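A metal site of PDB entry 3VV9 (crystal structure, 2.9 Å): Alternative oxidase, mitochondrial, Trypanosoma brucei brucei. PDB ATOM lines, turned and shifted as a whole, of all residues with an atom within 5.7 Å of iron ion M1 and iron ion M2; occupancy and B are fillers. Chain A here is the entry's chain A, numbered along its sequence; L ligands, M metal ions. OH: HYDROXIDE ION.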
ATOM      1  N   GLU A 123      22.579  -6.729  35.517  1.00  0.00           N
ATOM      2  CA  GLU A 123      22.531  -8.154  35.771  1.00  0.00           C
ATOM      3  C   GLU A 123      21.847  -8.533  37.099  1.00  0.00           C
ATOM      4  O   GLU A 123      21.347  -9.658  37.265  1.00  0.00           O
ATOM      5  CB  GLU A 123      23.932  -8.753  35.651  1.00  0.00           C
ATOM      6  CG  GLU A 123      24.640  -8.446  34.327  1.00  0.00           C
ATOM      7  CD  GLU A 123      23.965  -9.086  33.133  1.00  0.00           C
ATOM      8  OE1 GLU A 123      23.423  -8.326  32.301  1.00  0.00           O
ATOM      9  OE2 GLU A 123      23.944 -10.337  33.010  1.00  0.00           O
ATOM     10  N   ALA A 126      18.647  -8.548  35.769  1.00  0.00           N
ATOM     11  CA  ALA A 126      18.695  -9.474  34.600  1.00  0.00           C
ATOM     12  C   ALA A 126      18.279 -10.911  34.843  1.00  0.00           C
ATOM     13  O   ALA A 126      17.764 -11.559  33.936  1.00  0.00           O
ATOM     14  CB  ALA A 126      20.077  -9.450  33.961  1.00  0.00           C
ATOM     15  N   GLU A 158      17.773 -19.185  32.281  1.00  0.00           N
ATOM     16  CA  GLU A 158      17.922 -17.707  32.058  1.00  0.00           C
ATOM     17  C   GLU A 158      18.250 -16.997  33.368  1.00  0.00           C
ATOM     18  O   GLU A 158      19.129 -16.121  33.405  1.00  0.00           O
ATOM     19  CB  GLU A 158      16.700 -17.001  31.397  1.00  0.00           C
ATOM     20  CG  GLU A 158      16.302 -15.670  32.095  1.00  0.00           C
ATOM     21  CD  GLU A 158      15.554 -14.612  31.243  1.00  0.00           C
ATOM     22  OE1 GLU A 158      14.425 -14.895  30.750  1.00  0.00           O
ATOM     23  OE2 GLU A 158      16.069 -13.458  31.106  1.00  0.00           O
ATOM     24  N   GLU A 162      22.108 -15.564  33.772  1.00  0.00           N
ATOM     25  CA  GLU A 162      22.413 -14.161  34.078  1.00  0.00           C
ATOM     26  C   GLU A 162      23.036 -14.070  35.485  1.00  0.00           C
ATOM     27  O   GLU A 162      24.017 -13.346  35.683  1.00  0.00           O
ATOM     28  CB  GLU A 162      21.190 -13.227  33.938  1.00  0.00           C
ATOM     29  CG  GLU A 162      20.377 -13.376  32.637  1.00  0.00           C
ATOM     30  CD  GLU A 162      21.004 -12.773  31.367  1.00  0.00           C
ATOM     31  OE1 GLU A 162      22.195 -12.400  31.387  1.00  0.00           O
ATOM     32  OE2 GLU A 162      20.284 -12.695  30.320  1.00  0.00           O
ATOM     33  N   HIS A 165      26.516 -14.459  34.669  1.00  0.00           N
ATOM     34  CA  HIS A 165      26.923 -13.132  34.171  1.00  0.00           C
ATOM     35  C   HIS A 165      27.321 -12.191  35.332  1.00  0.00           C
ATOM     36  O   HIS A 165      28.285 -11.438  35.237  1.00  0.00           O
ATOM     37  CB  HIS A 165      25.765 -12.454  33.423  1.00  0.00           C
ATOM     38  CG  HIS A 165      25.505 -12.986  32.047  1.00  0.00           C
ATOM     39  ND1 HIS A 165      24.970 -12.191  31.043  1.00  0.00           N
ATOM     40  CD2 HIS A 165      25.725 -14.196  31.498  1.00  0.00           C
ATOM     41  CE1 HIS A 165      24.876 -12.902  29.941  1.00  0.00           C
ATOM     42  NE2 HIS A 165      25.318 -14.122  30.190  1.00  0.00           N
ATOM     43  N   LEU A 212      14.294  -6.111  26.429  1.00  0.00           N
ATOM     44  CA  LEU A 212      15.501  -5.895  27.248  1.00  0.00           C
ATOM     45  C   LEU A 212      16.688  -6.694  26.710  1.00  0.00           C
ATOM     46  O   LEU A 212      17.820  -6.270  26.866  1.00  0.00           O
ATOM     47  CB  LEU A 212      15.282  -6.246  28.709  1.00  0.00           C
ATOM     48  CG  LEU A 212      14.426  -5.359  29.634  1.00  0.00           C
ATOM     49  CD1 LEU A 212      14.411  -5.904  31.080  1.00  0.00           C
ATOM     50  CD2 LEU A 212      14.907  -3.916  29.593  1.00  0.00           C
ATOM     51  N   GLU A 213      16.426  -7.837  26.073  1.00  0.00           N
ATOM     52  CA  GLU A 213      17.500  -8.574  25.399  1.00  0.00           C
ATOM     53  C   GLU A 213      18.074  -7.868  24.162  1.00  0.00           C
ATOM     54  O   GLU A 213      19.265  -7.525  24.143  1.00  0.00           O
ATOM     55  CB  GLU A 213      17.080  -9.999  25.120  1.00  0.00           C
ATOM     56  CG  GLU A 213      16.960 -10.830  26.386  1.00  0.00           C
ATOM     57  CD  GLU A 213      18.195 -10.732  27.281  1.00  0.00           C
ATOM     58  OE1 GLU A 213      18.792  -9.620  27.389  1.00  0.00           O
ATOM     59  OE2 GLU A 213      18.562 -11.762  27.911  1.00  0.00           O
ATOM     60  N   ALA A 216      20.351  -5.617  25.282  1.00  0.00           N
ATOM     61  CA  ALA A 216      21.506  -6.309  25.840  1.00  0.00           C
ATOM     62  C   ALA A 216      22.492  -6.629  24.723  1.00  0.00           C
ATOM     63  O   ALA A 216      23.704  -6.351  24.858  1.00  0.00           O
ATOM     64  CB  ALA A 216      21.089  -7.577  26.546  1.00  0.00           C
ATOM     65  N   TYR A 220      26.244  -4.717  24.482  1.00  0.00           N
ATOM     66  CA  TYR A 220      27.475  -5.500  24.345  1.00  0.00           C
ATOM     67  C   TYR A 220      28.083  -5.440  22.959  1.00  0.00           C
ATOM     68  O   TYR A 220      29.307  -5.416  22.805  1.00  0.00           O
ATOM     69  CB  TYR A 220      27.251  -6.968  24.726  1.00  0.00           C
ATOM     70  CG  TYR A 220      26.902  -7.207  26.178  1.00  0.00           C
ATOM     71  CD1 TYR A 220      27.743  -6.795  27.207  1.00  0.00           C
ATOM     72  CD2 TYR A 220      25.721  -7.883  26.533  1.00  0.00           C
ATOM     73  CE1 TYR A 220      27.420  -7.020  28.539  1.00  0.00           C
ATOM     74  CE2 TYR A 220      25.385  -8.107  27.865  1.00  0.00           C
ATOM     75  CZ  TYR A 220      26.234  -7.675  28.863  1.00  0.00           C
ATOM     76  OH  TYR A 220      25.912  -7.915  30.156  1.00  0.00           O
ATOM     77  N   ILE A 262      28.804 -13.707  26.594  1.00  0.00           N
ATOM     78  CA  ILE A 262      27.838 -12.879  27.347  1.00  0.00           C
ATOM     79  C   ILE A 262      26.797 -12.287  26.397  1.00  0.00           C
ATOM     80  O   ILE A 262      25.600 -12.190  26.736  1.00  0.00           O
ATOM     81  CB  ILE A 262      28.483 -11.724  28.176  1.00  0.00           C
ATOM     82  CG1 ILE A 262      29.126 -12.247  29.471  1.00  0.00           C
ATOM     83  CG2 ILE A 262      27.451 -10.709  28.608  1.00  0.00           C
ATOM     84  CD1 ILE A 262      29.639 -11.153  30.379  1.00  0.00           C
ATOM     85  N   GLU A 266      22.795 -13.639  25.934  1.00  0.00           N
ATOM     86  CA  GLU A 266      21.730 -12.655  25.806  1.00  0.00           C
ATOM     87  C   GLU A 266      20.878 -12.850  24.547  1.00  0.00           C
ATOM     88  O   GLU A 266      19.670 -13.040  24.628  1.00  0.00           O
ATOM     89  CB  GLU A 266      22.266 -11.211  25.837  1.00  0.00           C
ATOM     90  CG  GLU A 266      22.951 -10.759  27.119  1.00  0.00           C
ATOM     91  CD  GLU A 266      22.127 -11.014  28.377  1.00  0.00           C
ATOM     92  OE1 GLU A 266      22.571 -10.569  29.442  1.00  0.00           O
ATOM     93  OE2 GLU A 266      21.054 -11.650  28.303  1.00  0.00           O
ATOM     94  N   HIS A 269      18.407 -15.582  24.835  1.00  0.00           N
ATOM     95  CA  HIS A 269      17.336 -15.114  25.702  1.00  0.00           C
ATOM     96  C   HIS A 269      16.338 -14.240  24.920  1.00  0.00           C
ATOM     97  O   HIS A 269      15.123 -14.362  25.098  1.00  0.00           O
ATOM     98  CB  HIS A 269      17.922 -14.406  26.910  1.00  0.00           C
ATOM     99  CG  HIS A 269      18.969 -15.200  27.629  1.00  0.00           C
ATOM    100  ND1 HIS A 269      20.183 -14.670  28.013  1.00  0.00           N
ATOM    101  CD2 HIS A 269      18.992 -16.509  28.020  1.00  0.00           C
ATOM    102  CE1 HIS A 269      20.902 -15.611  28.609  1.00  0.00           C
ATOM    103  NE2 HIS A 269      20.202 -16.727  28.629  1.00  0.00           N
HETATM  104  O    OH L   1      22.254  -8.050  30.329  1.00  0.00           O
HETATM  105 FE    FE M   1      19.671 -10.584  29.534  1.00  0.00          FE
HETATM  106 FE    FE M   2      22.630  -9.915  31.297  1.00  0.00          FE
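Ala 126 touches iron ion M2 (CB to FE, 3.7 Å).
ND1 of His 165 touches iron ion M2, 3.3 Å away.
OE2 of Glu 266 is bound to iron ion M1, 2.1 Å away.
Iron ion M1 is bound by OE2 of Glu 213, at 2.3 Å.
Iron ion M1 is bound by OE2 of Glu 162, 2.3 Å away.
Iron ion M1 is bound by OE1 of Glu 213 (2.5 Å).
Iron ion M1 has four donor atoms within binding distance.
Iron ion M2 is bound by the side-chain carboxylate (OE1) of Glu 266 (2.0 Å), the side-chain carboxylate (OE1) of Glu 123 (2.0 Å), an oxygen (O) of the ligand (2.1 Å), the side-chain carboxylate (OE2) of Glu 123 (2.2 Å) and the side-chain carboxylate (OE1) of Glu 162 (2.5 Å).
Within 4 Å of iron ion M1: Glu 162, Glu 213 and Glu 266.
ND1 of His 165 lies close to OE1 of Glu 266 (3.3 Å).
ND1 of His 269 sits close to N of Glu 266, at 3.5 Å.
ND1 of His 165 sits close to OE2 of Glu 123 (2.9 Å).
OE1 of Glu 123 lies close to OH of Tyr 220 (3.3 Å).
ND1 of His 269 sits close to OE2 of Glu 213, 3.3 Å away.
A ring nitrogen (ND1) of His 165 lies close to the side-chain carboxylate (OE1) of Glu 162.
The side-chain carboxylate of Glu 162 lies close to a ring nitrogen (ND1) of His 269, 3.0 Å away.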
